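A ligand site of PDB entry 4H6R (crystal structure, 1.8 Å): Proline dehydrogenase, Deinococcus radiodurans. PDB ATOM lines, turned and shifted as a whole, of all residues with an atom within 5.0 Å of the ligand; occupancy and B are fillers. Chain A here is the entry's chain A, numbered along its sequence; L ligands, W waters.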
ATOM      1  N   ARG A  35      18.137   4.390 -16.196  1.00  0.00           N
ATOM      2  CA  ARG A  35      18.842   4.087 -14.950  1.00  0.00           C
ATOM      3  C   ARG A  35      17.904   3.724 -13.789  1.00  0.00           C
ATOM      4  O   ARG A  35      18.243   2.900 -12.918  1.00  0.00           O
ATOM      5  CB  ARG A  35      19.746   5.271 -14.574  1.00  0.00           C
ATOM      6  CG  ARG A  35      20.303   5.161 -13.160  1.00  0.00           C
ATOM      7  CD  ARG A  35      21.378   6.236 -12.893  1.00  0.00           C
ATOM      8  NE  ARG A  35      21.708   6.256 -11.459  1.00  0.00           N
ATOM      9  CZ  ARG A  35      22.216   7.302 -10.821  1.00  0.00           C
ATOM     10  NH1 ARG A  35      22.500   8.420 -11.482  1.00  0.00           N
ATOM     11  NH2 ARG A  35      22.442   7.221  -9.518  1.00  0.00           N
ATOM     12  N   PHE A  36      16.700   4.312 -13.776  1.00  0.00           N
ATOM     13  CA  PHE A  36      15.835   4.264 -12.632  1.00  0.00           C
ATOM     14  C   PHE A  36      14.549   3.511 -12.907  1.00  0.00           C
ATOM     15  O   PHE A  36      13.827   3.224 -11.975  1.00  0.00           O
ATOM     16  CB  PHE A  36      15.435   5.693 -12.213  1.00  0.00           C
ATOM     17  CG  PHE A  36      16.604   6.597 -11.903  1.00  0.00           C
ATOM     18  CD1 PHE A  36      17.340   6.442 -10.726  1.00  0.00           C
ATOM     19  CD2 PHE A  36      16.943   7.631 -12.771  1.00  0.00           C
ATOM     20  CE1 PHE A  36      18.420   7.304 -10.435  1.00  0.00           C
ATOM     21  CE2 PHE A  36      18.015   8.500 -12.488  1.00  0.00           C
ATOM     22  CZ  PHE A  36      18.758   8.323 -11.312  1.00  0.00           C
ATOM     23  N   ASN A  60      11.227  -5.945  -6.409  1.00  0.00           N
ATOM     24  CA  ASN A  60      10.037  -5.398  -5.776  1.00  0.00           C
ATOM     25  C   ASN A  60       9.442  -4.515  -6.877  1.00  0.00           C
ATOM     26  O   ASN A  60       9.968  -3.442  -7.168  1.00  0.00           O
ATOM     27  CB  ASN A  60      10.479  -4.596  -4.550  1.00  0.00           C
ATOM     28  CG  ASN A  60       9.332  -3.883  -3.865  1.00  0.00           C
ATOM     29  OD1 ASN A  60       8.184  -3.997  -4.275  1.00  0.00           O
ATOM     30  ND2 ASN A  60       9.644  -3.230  -2.751  1.00  0.00           N
ATOM     31  N   ASP A 137       2.246   0.766  -0.212  1.00  0.00           N
ATOM     32  CA  ASP A 137       3.146   1.896  -0.005  1.00  0.00           C
ATOM     33  C   ASP A 137       2.412   2.962   0.787  1.00  0.00           C
ATOM     34  O   ASP A 137       1.183   3.058   0.748  1.00  0.00           O
ATOM     35  CB  ASP A 137       3.598   2.490  -1.338  1.00  0.00           C
ATOM     36  CG  ASP A 137       4.682   1.656  -2.025  1.00  0.00           C
ATOM     37  OD1 ASP A 137       5.113   0.634  -1.456  1.00  0.00           O
ATOM     38  OD2 ASP A 137       5.084   2.047  -3.133  1.00  0.00           O
ATOM     39  N   MET A 138       3.160   3.838   1.439  1.00  0.00           N
ATOM     40  CA  MET A 138       2.492   4.906   2.191  1.00  0.00           C
ATOM     41  C   MET A 138       2.582   6.216   1.441  1.00  0.00           C
ATOM     42  O   MET A 138       3.666   6.600   0.973  1.00  0.00           O
ATOM     43  CB  MET A 138       3.082   5.029   3.605  1.00  0.00           C
ATOM     44  CG  MET A 138       2.290   5.987   4.525  1.00  0.00           C
ATOM     45  SD  MET A 138       0.666   5.314   4.913  1.00  0.00           S
ATOM     46  CE  MET A 138       1.089   3.893   5.977  1.00  0.00           C
ATOM     47  N   VAL A 166       4.329   0.302   4.909  1.00  0.00           N
ATOM     48  CA  VAL A 166       5.474   1.231   4.974  1.00  0.00           C
ATOM     49  C   VAL A 166       5.218   2.235   6.040  1.00  0.00           C
ATOM     50  O   VAL A 166       4.084   2.690   6.183  1.00  0.00           O
ATOM     51  CB  VAL A 166       5.591   2.027   3.608  1.00  0.00           C
ATOM     52  CG1 VAL A 166       6.701   3.104   3.681  1.00  0.00           C
ATOM     53  CG2 VAL A 166       5.817   1.063   2.443  1.00  0.00           C
ATOM     54  N   GLN A 168       6.948   6.016   7.493  1.00  0.00           N
ATOM     55  CA  GLN A 168       7.857   7.099   7.134  1.00  0.00           C
ATOM     56  C   GLN A 168       8.420   7.800   8.353  1.00  0.00           C
ATOM     57  O   GLN A 168       7.662   8.285   9.237  1.00  0.00           O
ATOM     58  CB  GLN A 168       7.099   8.131   6.293  1.00  0.00           C
ATOM     59  CG  GLN A 168       6.490   7.566   5.014  1.00  0.00           C
ATOM     60  CD  GLN A 168       5.194   8.263   4.665  1.00  0.00           C
ATOM     61  OE1 GLN A 168       4.402   8.556   5.549  1.00  0.00           O
ATOM     62  NE2 GLN A 168       4.939   8.490   3.363  1.00  0.00           N
ATOM     63  N   TYR A 170       9.900  10.568   8.802  1.00  0.00           N
ATOM     64  CA  TYR A 170       9.699  12.017   9.021  1.00  0.00           C
ATOM     65  C   TYR A 170       8.429  12.400   9.780  1.00  0.00           C
ATOM     66  O   TYR A 170       8.342  13.499  10.263  1.00  0.00           O
ATOM     67  CB  TYR A 170       9.893  12.879   7.750  1.00  0.00           C
ATOM     68  CG  TYR A 170       8.893  12.684   6.608  1.00  0.00           C
ATOM     69  CD1 TYR A 170       9.044  13.413   5.418  1.00  0.00           C
ATOM     70  CD2 TYR A 170       7.828  11.789   6.701  1.00  0.00           C
ATOM     71  CE1 TYR A 170       8.158  13.263   4.365  1.00  0.00           C
ATOM     72  CE2 TYR A 170       6.935  11.618   5.648  1.00  0.00           C
ATOM     73  CZ  TYR A 170       7.103  12.365   4.480  1.00  0.00           C
ATOM     74  OH  TYR A 170       6.221  12.199   3.408  1.00  0.00           O
ATOM     75  N   ARG A 189       8.208  -1.794   5.809  1.00  0.00           N
ATOM     76  CA  ARG A 189       9.357  -1.109   5.216  1.00  0.00           C
ATOM     77  C   ARG A 189       9.492   0.256   5.864  1.00  0.00           C
ATOM     78  O   ARG A 189       8.541   1.019   5.856  1.00  0.00           O
ATOM     79  CB  ARG A 189       9.083  -0.957   3.686  1.00  0.00           C
ATOM     80  CG  ARG A 189      10.190  -0.159   2.964  1.00  0.00           C
ATOM     81  CD  ARG A 189       9.750   0.404   1.593  1.00  0.00           C
ATOM     82  NE  ARG A 189       9.264  -0.711   0.772  1.00  0.00           N
ATOM     83  CZ  ARG A 189       8.284  -0.639  -0.131  1.00  0.00           C
ATOM     84  NH1 ARG A 189       7.912  -1.763  -0.771  1.00  0.00           N
ATOM     85  NH2 ARG A 189       7.650   0.518  -0.377  1.00  0.00           N
ATOM     86  N   VAL A 191      10.971   3.975   5.644  1.00  0.00           N
ATOM     87  CA  VAL A 191      11.551   4.890   4.660  1.00  0.00           C
ATOM     88  C   VAL A 191      11.656   6.233   5.342  1.00  0.00           C
ATOM     89  O   VAL A 191      11.043   6.444   6.363  1.00  0.00           O
ATOM     90  CB  VAL A 191      10.638   5.049   3.395  1.00  0.00           C
ATOM     91  CG1 VAL A 191      10.460   3.693   2.751  1.00  0.00           C
ATOM     92  CG2 VAL A 191       9.276   5.678   3.793  1.00  0.00           C
ATOM     93  N   LYS A 192      12.462   7.138   4.809  1.00  0.00           N
ATOM     94  CA  LYS A 192      12.512   8.446   5.458  1.00  0.00           C
ATOM     95  C   LYS A 192      11.224   9.261   5.212  1.00  0.00           C
ATOM     96  O   LYS A 192      10.767  10.019   6.073  1.00  0.00           O
ATOM     97  CB  LYS A 192      13.745   9.205   4.949  1.00  0.00           C
ATOM     98  CG  LYS A 192      15.057   8.704   5.607  1.00  0.00           C
ATOM     99  CD  LYS A 192      16.234   9.622   5.309  1.00  0.00           C
ATOM    100  CE  LYS A 192      17.553   8.942   5.671  1.00  0.00           C
ATOM    101  NZ  LYS A 192      18.686   9.968   5.517  1.00  0.00           N
ATOM    102  N   GLY A 193      10.682   9.118   4.023  1.00  0.00           N
ATOM    103  CA  GLY A 193       9.524   9.877   3.648  1.00  0.00           C
ATOM    104  C   GLY A 193       9.711  10.663   2.366  1.00  0.00           C
ATOM    105  O   GLY A 193      10.692  11.381   2.231  1.00  0.00           O
ATOM    106  N   ALA A 194       8.730  10.594   1.450  1.00  0.00           N
ATOM    107  CA  ALA A 194       8.931  11.161   0.111  1.00  0.00           C
ATOM    108  C   ALA A 194       8.154  12.444  -0.178  1.00  0.00           C
ATOM    109  O   ALA A 194       8.410  13.087  -1.197  1.00  0.00           O
ATOM    110  CB  ALA A 194       8.636  10.124  -0.960  1.00  0.00           C
ATOM    111  N   TYR A 195       7.224  12.810   0.695  1.00  0.00           N
ATOM    112  CA  TYR A 195       6.305  13.912   0.359  1.00  0.00           C
ATOM    113  C   TYR A 195       6.695  15.231   0.984  1.00  0.00           C
ATOM    114  O   TYR A 195       7.486  15.296   1.922  1.00  0.00           O
ATOM    115  CB  TYR A 195       4.850  13.535   0.691  1.00  0.00           C
ATOM    116  CG  TYR A 195       4.366  12.332  -0.079  1.00  0.00           C
ATOM    117  CD1 TYR A 195       3.623  12.490  -1.248  1.00  0.00           C
ATOM    118  CD2 TYR A 195       4.688  11.039   0.326  1.00  0.00           C
ATOM    119  CE1 TYR A 195       3.201  11.375  -1.982  1.00  0.00           C
ATOM    120  CE2 TYR A 195       4.259   9.936  -0.403  1.00  0.00           C
ATOM    121  CZ  TYR A 195       3.500  10.114  -1.539  1.00  0.00           C
ATOM    122  OH  TYR A 195       3.077   9.001  -2.236  1.00  0.00           O
ATOM    123  N   ALA A 230      14.694   0.418   3.944  1.00  0.00           N
ATOM    124  CA  ALA A 230      14.667   1.059   2.614  1.00  0.00           C
ATOM    125  C   ALA A 230      15.301   2.422   2.677  1.00  0.00           C
ATOM    126  O   ALA A 230      14.654   3.403   3.094  1.00  0.00           O
ATOM    127  CB  ALA A 230      13.203   1.181   2.112  1.00  0.00           C
ATOM    128  N   THR A 231      16.585   2.486   2.324  1.00  0.00           N
ATOM    129  CA  THR A 231      17.323   3.736   2.409  1.00  0.00           C
ATOM    130  C   THR A 231      18.564   3.589   1.575  1.00  0.00           C
ATOM    131  O   THR A 231      19.033   2.451   1.388  1.00  0.00           O
ATOM    132  CB  THR A 231      17.728   4.090   3.887  1.00  0.00           C
ATOM    133  OG1 THR A 231      18.441   5.330   3.851  1.00  0.00           O
ATOM    134  CG2 THR A 231      18.651   3.003   4.496  1.00  0.00           C
ATOM    135  N   HIS A 232      19.115   4.700   1.072  1.00  0.00           N
ATOM    136  CA  HIS A 232      20.391   4.674   0.373  1.00  0.00           C
ATOM    137  C   HIS A 232      21.457   5.418   1.181  1.00  0.00           C
ATOM    138  O   HIS A 232      22.527   5.712   0.662  1.00  0.00           O
ATOM    139  CB  HIS A 232      20.275   5.367  -0.976  1.00  0.00           C
ATOM    140  CG  HIS A 232      19.045   4.975  -1.710  1.00  0.00           C
ATOM    141  ND1 HIS A 232      17.840   5.614  -1.504  1.00  0.00           N
ATOM    142  CD2 HIS A 232      18.805   3.949  -2.560  1.00  0.00           C
ATOM    143  CE1 HIS A 232      16.911   5.035  -2.250  1.00  0.00           C
ATOM    144  NE2 HIS A 232      17.477   4.040  -2.921  1.00  0.00           N
ATOM    145  N   ASP A 233      21.111   5.778   2.421  1.00  0.00           N
ATOM    146  CA  ASP A 233      21.998   6.554   3.326  1.00  0.00           C
ATOM    147  C   ASP A 233      23.034   5.577   3.927  1.00  0.00           C
ATOM    148  O   ASP A 233      22.699   4.705   4.740  1.00  0.00           O
ATOM    149  CB  ASP A 233      21.097   7.189   4.407  1.00  0.00           C
ATOM    150  CG  ASP A 233      21.883   8.015   5.453  1.00  0.00           C
ATOM    151  OD1 ASP A 233      23.064   7.721   5.731  1.00  0.00           O
ATOM    152  OD2 ASP A 233      21.301   8.985   6.015  1.00  0.00           O
ATOM    153  N   GLN A 257      16.570  -2.387   1.320  1.00  0.00           N
ATOM    154  CA  GLN A 257      15.864  -2.107   0.067  1.00  0.00           C
ATOM    155  C   GLN A 257      16.355  -0.801  -0.538  1.00  0.00           C
ATOM    156  O   GLN A 257      16.656   0.146   0.187  1.00  0.00           O
ATOM    157  CB  GLN A 257      14.348  -2.059   0.259  1.00  0.00           C
ATOM    158  CG  GLN A 257      13.792  -3.459   0.618  1.00  0.00           C
ATOM    159  CD  GLN A 257      12.297  -3.456   0.567  1.00  0.00           C
ATOM    160  OE1 GLN A 257      11.683  -2.390   0.491  1.00  0.00           O
ATOM    161  NE2 GLN A 257      11.680  -4.645   0.677  1.00  0.00           N
ATOM    162  N   MET A 258      16.514  -0.788  -1.859  1.00  0.00           N
ATOM    163  CA  MET A 258      17.000   0.438  -2.549  1.00  0.00           C
ATOM    164  C   MET A 258      16.172   0.625  -3.806  1.00  0.00           C
ATOM    165  O   MET A 258      15.630  -0.365  -4.330  1.00  0.00           O
ATOM    166  CB  MET A 258      18.492   0.345  -2.904  1.00  0.00           C
ATOM    167  CG  MET A 258      19.318   0.420  -1.682  1.00  0.00           C
ATOM    168  SD  MET A 258      19.660  -1.280  -1.174  1.00  0.00           S
ATOM    169  CE  MET A 258      20.886  -0.864   0.056  1.00  0.00           C
ATOM    170  N   LEU A 259      16.088   1.862  -4.295  1.00  0.00           N
ATOM    171  CA  LEU A 259      15.481   2.109  -5.604  1.00  0.00           C
ATOM    172  C   LEU A 259      16.447   1.687  -6.720  1.00  0.00           C
ATOM    173  O   LEU A 259      17.670   1.854  -6.617  1.00  0.00           O
ATOM    174  CB  LEU A 259      15.155   3.611  -5.784  1.00  0.00           C
ATOM    175  CG  LEU A 259      14.202   4.154  -4.718  1.00  0.00           C
ATOM    176  CD1 LEU A 259      13.950   5.634  -4.977  1.00  0.00           C
ATOM    177  CD2 LEU A 259      12.863   3.369  -4.726  1.00  0.00           C
ATOM    178  N   ILE A 262      20.064   3.410  -7.765  1.00  0.00           N
ATOM    179  CA  ILE A 262      20.660   4.278  -6.750  1.00  0.00           C
ATOM    180  C   ILE A 262      21.516   3.419  -5.816  1.00  0.00           C
ATOM    181  O   ILE A 262      21.025   2.456  -5.190  1.00  0.00           O
ATOM    182  CB  ILE A 262      19.620   5.003  -5.920  1.00  0.00           C
ATOM    183  CG1 ILE A 262      18.680   5.818  -6.842  1.00  0.00           C
ATOM    184  CG2 ILE A 262      20.311   5.935  -4.887  1.00  0.00           C
ATOM    185  CD1 ILE A 262      17.591   6.531  -6.008  1.00  0.00           C
ATOM    186  N   ARG A 263      22.794   3.816  -5.760  1.00  0.00           N
ATOM    187  CA  ARG A 263      23.842   3.097  -5.014  1.00  0.00           C
ATOM    188  C   ARG A 263      23.884   1.640  -5.393  1.00  0.00           C
ATOM    189  O   ARG A 263      23.851   0.761  -4.524  1.00  0.00           O
ATOM    190  CB  ARG A 263      23.698   3.245  -3.491  1.00  0.00           C
ATOM    191  CG  ARG A 263      23.900   4.706  -3.014  1.00  0.00           C
ATOM    192  CD  ARG A 263      25.269   5.282  -3.429  1.00  0.00           C
ATOM    193  NE  ARG A 263      26.437   4.477  -3.033  1.00  0.00           N
ATOM    194  CZ  ARG A 263      27.143   4.655  -1.895  1.00  0.00           C
ATOM    195  NH1 ARG A 263      26.775   5.573  -1.010  1.00  0.00           N
ATOM    196  NH2 ARG A 263      28.219   3.886  -1.633  1.00  0.00           N
ATOM    197  N   TYR A 280      13.612  -1.969  -5.576  1.00  0.00           N
ATOM    198  CA  TYR A 280      12.328  -1.482  -6.053  1.00  0.00           C
ATOM    199  C   TYR A 280      12.468  -1.128  -7.523  1.00  0.00           C
ATOM    200  O   TYR A 280      13.356  -0.334  -7.895  1.00  0.00           O
ATOM    201  CB  TYR A 280      12.044  -0.217  -5.250  1.00  0.00           C
ATOM    202  CG  TYR A 280      10.663   0.328  -5.272  1.00  0.00           C
ATOM    203  CD1 TYR A 280       9.722  -0.062  -4.327  1.00  0.00           C
ATOM    204  CD2 TYR A 280      10.320   1.347  -6.162  1.00  0.00           C
ATOM    205  CE1 TYR A 280       8.451   0.501  -4.281  1.00  0.00           C
ATOM    206  CE2 TYR A 280       9.055   1.940  -6.120  1.00  0.00           C
ATOM    207  CZ  TYR A 280       8.122   1.510  -5.170  1.00  0.00           C
ATOM    208  OH  TYR A 280       6.851   2.082  -5.127  1.00  0.00           O
ATOM    209  N   ARG A 293      11.362  12.784  -9.875  1.00  0.00           N
ATOM    210  CA  ARG A 293      11.706  12.804  -8.443  1.00  0.00           C
ATOM    211  C   ARG A 293      13.122  12.291  -8.233  1.00  0.00           C
ATOM    212  O   ARG A 293      13.814  12.744  -7.312  1.00  0.00           O
ATOM    213  CB  ARG A 293      10.704  12.013  -7.589  1.00  0.00           C
ATOM    214  CG  ARG A 293       9.323  12.685  -7.413  1.00  0.00           C
ATOM    215  CD  ARG A 293       9.448  14.161  -6.973  1.00  0.00           C
ATOM    216  NE  ARG A 293      10.166  14.286  -5.707  1.00  0.00           N
ATOM    217  CZ  ARG A 293      10.765  15.387  -5.273  1.00  0.00           C
ATOM    218  NH1 ARG A 293      11.399  15.382  -4.101  1.00  0.00           N
ATOM    219  NH2 ARG A 293      10.738  16.505  -6.009  1.00  0.00           N
ATOM    220  N   ARG A 294      13.565  11.336  -9.050  1.00  0.00           N
ATOM    221  CA  ARG A 294      14.955  10.884  -8.969  1.00  0.00           C
ATOM    222  C   ARG A 294      15.907  12.015  -9.320  1.00  0.00           C
ATOM    223  O   ARG A 294      16.925  12.202  -8.629  1.00  0.00           O
ATOM    224  CB  ARG A 294      15.187   9.717  -9.917  1.00  0.00           C
ATOM    225  CG  ARG A 294      14.256   8.498  -9.615  1.00  0.00           C
ATOM    226  CD  ARG A 294      14.481   7.835  -8.255  1.00  0.00           C
ATOM    227  NE  ARG A 294      13.944   8.543  -7.079  1.00  0.00           N
ATOM    228  CZ  ARG A 294      12.650   8.692  -6.780  1.00  0.00           C
ATOM    229  NH1 ARG A 294      11.707   8.215  -7.565  1.00  0.00           N
ATOM    230  NH2 ARG A 294      12.294   9.320  -5.687  1.00  0.00           N
ATOM    231  N   ILE A 295      15.603  12.743 -10.397  1.00  0.00           N
ATOM    232  CA  ILE A 295      16.361  13.946 -10.751  1.00  0.00           C
ATOM    233  C   ILE A 295      16.410  14.971  -9.609  1.00  0.00           C
ATOM    234  O   ILE A 295      17.479  15.490  -9.269  1.00  0.00           O
ATOM    235  CB  ILE A 295      15.818  14.634 -12.042  1.00  0.00           C
ATOM    236  CG1 ILE A 295      15.932  13.695 -13.237  1.00  0.00           C
ATOM    237  CG2 ILE A 295      16.558  15.967 -12.316  1.00  0.00           C
ATOM    238  CD1 ILE A 295      15.360  14.317 -14.533  1.00  0.00           C
ATOM    239  N   GLU A 297      16.270  14.618  -6.514  1.00  0.00           N
ATOM    240  CA  GLU A 297      16.976  14.139  -5.323  1.00  0.00           C
ATOM    241  C   GLU A 297      18.448  13.844  -5.585  1.00  0.00           C
ATOM    242  O   GLU A 297      19.136  13.248  -4.751  1.00  0.00           O
ATOM    243  CB  GLU A 297      16.244  12.915  -4.748  1.00  0.00           C
ATOM    244  N   THR A 298      18.957  14.279  -6.737  1.00  0.00           N
ATOM    245  CA  THR A 298      20.363  14.155  -7.046  1.00  0.00           C
ATOM    246  C   THR A 298      21.222  14.911  -6.002  1.00  0.00           C
ATOM    247  O   THR A 298      20.984  16.104  -5.754  1.00  0.00           O
ATOM    248  CB  THR A 298      20.654  14.773  -8.408  1.00  0.00           C
ATOM    249  OG1 THR A 298      19.844  14.129  -9.406  1.00  0.00           O
ATOM    250  CG2 THR A 298      22.128  14.645  -8.741  1.00  0.00           C
ATOM    251  N   PRO A 299      22.239  14.235  -5.409  1.00  0.00           N
ATOM    252  CA  PRO A 299      23.020  14.844  -4.319  1.00  0.00           C
ATOM    253  C   PRO A 299      24.032  15.897  -4.758  1.00  0.00           C
ATOM    254  O   PRO A 299      24.323  16.011  -5.952  1.00  0.00           O
ATOM    255  CB  PRO A 299      23.747  13.647  -3.690  1.00  0.00           C
ATOM    256  CG  PRO A 299      23.880  12.658  -4.818  1.00  0.00           C
ATOM    257  CD  PRO A 299      22.615  12.829  -5.659  1.00  0.00           C
HETATM  258  P1  LIG L   1      18.435  10.606   1.648  1.00  0.00           P
HETATM  259  O1  LIG L   1      17.256  11.298   0.937  1.00  0.00           O
HETATM  260  O2  LIG L   1      19.089  11.136   2.842  1.00  0.00           O
HETATM  261  O3  LIG L   1      19.581  10.230   0.738  1.00  0.00           O
HETATM  262  C1  LIG L   1      20.749   9.549   1.191  1.00  0.00           C
HETATM  263  C2  LIG L   1      21.711   9.339   0.013  1.00  0.00           C
HETATM  264  O4  LIG L   1      21.240   8.464  -0.981  1.00  0.00           O
HETATM  265  C3  LIG L   1      21.991  10.577  -0.763  1.00  0.00           C
HETATM  266  O5  LIG L   1      22.880  11.339  -0.034  1.00  0.00           O
HETATM  267  C4  LIG L   1      22.536  10.011  -2.025  1.00  0.00           C
HETATM  268  O6  LIG L   1      23.847   9.577  -1.841  1.00  0.00           O
HETATM  269  C5  LIG L   1      21.697   8.795  -2.249  1.00  0.00           C
HETATM  270  N1  LIG L   1      20.517   9.123  -3.042  1.00  0.00           N
HETATM  271  C6  LIG L   1      19.212   9.246  -2.627  1.00  0.00           C
HETATM  272  N2  LIG L   1      18.432   9.593  -3.658  1.00  0.00           N
HETATM  273  C7  LIG L   1      19.224   9.688  -4.807  1.00  0.00           C
HETATM  274  C8  LIG L   1      18.993  10.024  -6.134  1.00  0.00           C
HETATM  275  N3  LIG L   1      17.677  10.315  -6.593  1.00  0.00           N
HETATM  276  N4  LIG L   1      19.998  10.052  -7.006  1.00  0.00           N
HETATM  277  C9  LIG L   1      21.265   9.760  -6.637  1.00  0.00           C
HETATM  278  N5  LIG L   1      21.540   9.446  -5.347  1.00  0.00           N
HETATM  279  C10 LIG L   1      20.564   9.415  -4.425  1.00  0.00           C
HETATM  280  N6  LIG L   1       8.710   7.082   0.491  1.00  0.00           N
HETATM  281  C11 LIG L   1       7.362   7.163   0.949  1.00  0.00           C
HETATM  282  O7  LIG L   1       6.930   8.281   1.521  1.00  0.00           O
HETATM  283  N7  LIG L   1       6.448   6.121   0.850  1.00  0.00           N
HETATM  284  C12 LIG L   1       6.859   4.938   0.280  1.00  0.00           C
HETATM  285  O8  LIG L   1       6.002   3.930   0.177  1.00  0.00           O
HETATM  286  C13 LIG L   1       8.229   4.811  -0.226  1.00  0.00           C
HETATM  287  N8  LIG L   1       8.615   3.574  -0.865  1.00  0.00           N
HETATM  288  C14 LIG L   1      10.031   3.427  -1.018  1.00  0.00           C
HETATM  289  C15 LIG L   1      10.525   2.070  -1.332  1.00  0.00           C
HETATM  290  C16 LIG L   1      11.927   1.917  -1.337  1.00  0.00           C
HETATM  291  C17 LIG L   1      12.455   0.525  -1.667  1.00  0.00           C
HETATM  292  C18 LIG L   1      12.805   2.994  -1.095  1.00  0.00           C
HETATM  293  C19 LIG L   1      14.304   2.776  -1.123  1.00  0.00           C
HETATM  294  C20 LIG L   1      12.337   4.305  -0.799  1.00  0.00           C
HETATM  295  C21 LIG L   1      10.889   4.463  -0.766  1.00  0.00           C
HETATM  296  N9  LIG L   1      10.428   5.772  -0.478  1.00  0.00           N
HETATM  297  C22 LIG L   1       9.083   5.850  -0.095  1.00  0.00           C
HETATM  298  C23 LIG L   1      11.254   6.996  -0.616  1.00  0.00           C
HETATM  299  C24 LIG L   1      11.879   7.356   0.708  1.00  0.00           C
HETATM  300  O9  LIG L   1      10.881   7.921   1.525  1.00  0.00           O
HETATM  301  C25 LIG L   1      13.016   8.324   0.572  1.00  0.00           C
HETATM  302  O10 LIG L   1      12.476   9.451  -0.047  1.00  0.00           O
HETATM  303  C26 LIG L   1      14.176   7.813  -0.302  1.00  0.00           C
HETATM  304  O11 LIG L   1      14.558   6.524   0.070  1.00  0.00           O
HETATM  305  C27 LIG L   1      15.432   8.718  -0.171  1.00  0.00           C
HETATM  306  O12 LIG L   1      15.836   8.684   1.180  1.00  0.00           O
HETATM  307  P2  LIG L   1      17.151   8.010   1.759  1.00  0.00           P
HETATM  308  O13 LIG L   1      16.856   6.974   2.869  1.00  0.00           O
HETATM  309  O14 LIG L   1      17.908   7.456   0.530  1.00  0.00           O
HETATM  310  O15 LIG L   1      18.113   9.255   2.280  1.00  0.00           O
HETATM  311  O   HOH W   1      20.211  11.428  -9.458  1.00  0.00           O
HETATM  312  O   HOH W   2      15.109  12.300   2.268  1.00  0.00           O
HETATM  313  O   HOH W   3      14.356   6.109   2.886  1.00  0.00           O
HETATM  314  O   HOH W   4      23.960   8.309  -5.062  1.00  0.00           O
HETATM  315  O   HOH W   5      19.714  12.667  -2.228  1.00  0.00           O
HETATM  316  O   HOH W   6      24.404   7.218  -0.514  1.00  0.00           O
HETATM  317  O   HOH W   7      12.527  -2.828  -2.573  1.00  0.00           O
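O10 of the ligand is in hydrogen-bond range of O of Gly 193 (3.5 Å). N3 of the ligand is in hydrogen-bond range of O of Arg 294, at 2.9 Å. A ring nitrogen (ND1) of His 232 lies within hydrogen-bond range of an oxygen (O14) of the ligand (2.7 Å). An oxygen (O8) of the ligand sits at hydrogen-bond distance from the backbone NH of Met 138 (3.1 Å). NE2 of Gln 168 lies within hydrogen-bond range of O7 of the ligand. The backbone NH (N) of Ala 194 is in hydrogen-bond range of an oxygen (O7) of the ligand (2.9 Å). An oxygen (O2) of the ligand lies within salt-bridge range of the side-chain amino group (NZ) of Lys 192 (2.9 Å). The backbone NH (N) of His 232 is in hydrogen-bond range of an oxygen (O14) of the ligand (3.1 Å). N of Gly 193 sits at hydrogen-bond distance from O9 of the ligand (2.8 Å). N7 of the ligand is in hydrogen-bond range of O of Met 138 (2.8 Å). The side-chain hydroxyl (OG1) of Thr 231 sits at hydrogen-bond distance from an oxygen (O13) of the ligand, 2.5 Å away.
The guanidinium group of Arg 189 is in hydrogen-bond range of the side-chain amide oxygen of Gln 257. A ring nitrogen (NE2) of His 232 is in hydrogen-bond range of the backbone NH (N) of Leu 259, 2.9 Å away. The side-chain hydroxyl (OH) of Tyr 280 is in hydrogen-bond range of the side-chain carboxylate (OD2) of Asp 137, at 2.7 Å. The guanidinium group of Arg 189 sits close to the side-chain amide nitrogen of Asn 60 (3.0 Å). The backbone NH (N) of Tyr 280 lies within hydrogen-bond range of the backbone carbonyl oxygen (O) of Met 258, 2.9 Å away. O of Met 138 sits at hydrogen-bond distance from NE2 of Gln 168 (3.3 Å). The side-chain carboxylate of Asp 137 is in salt-bridge range of the guanidinium group of Arg 189 (2.8 Å). O of Gln 257 sits at hydrogen-bond distance from N of Thr 231 (3.2 Å).
NH2 of Arg 189 lies close to N8 of the ligand, at 3.2 Å. Residues that only touch the ligand: Asp 137, Val 166, Val 191, Tyr 195, Ala 230, Asp 233, Gln 257, Met 258, Leu 259, Ile 262, Tyr 280, Glu 297 and Pro 299. Hydrophobic or aromatic side chains within 4 Å of the ligand: Val 166, Val 191, Ala 194, Tyr 195, Ala 230, His 232, Leu 259, Ile 262, Tyr 280 and Pro 299. Of the 30 residues printed, 22 come within 4 Å of the ligand. The nearest printed residue that does not touch the ligand is Arg 35 (4.02 Å).
Water W3 lies within hydrogen-bond range of an oxygen (O13) of the ligand (2.6 Å), the backbone carbonyl oxygen (O) of Ala 230 (2.7 Å) and the backbone NH (N) of Lys 192 (2.9 Å). Water W6 lies within hydrogen-bond range of the backbone carbonyl oxygen of His 232 (2.7 Å), an oxygen (O6) of the ligand (2.8 Å) and the guanidinium group of Arg 263 (2.9 Å). Water W1 lies within hydrogen-bond range of the side-chain hydroxyl of Thr 298 (2.7 Å), a nitrogen (N4) of the ligand (2.8 Å) and the backbone carbonyl oxygen of Arg 294 (3.5 Å). Water W7 lies within hydrogen-bond range of the side-chain amide nitrogen of Asn 60 (2.9 Å), the side-chain amide oxygen of Gln 257 (3.2 Å) and the backbone NH of Tyr 280 (3.3 Å).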
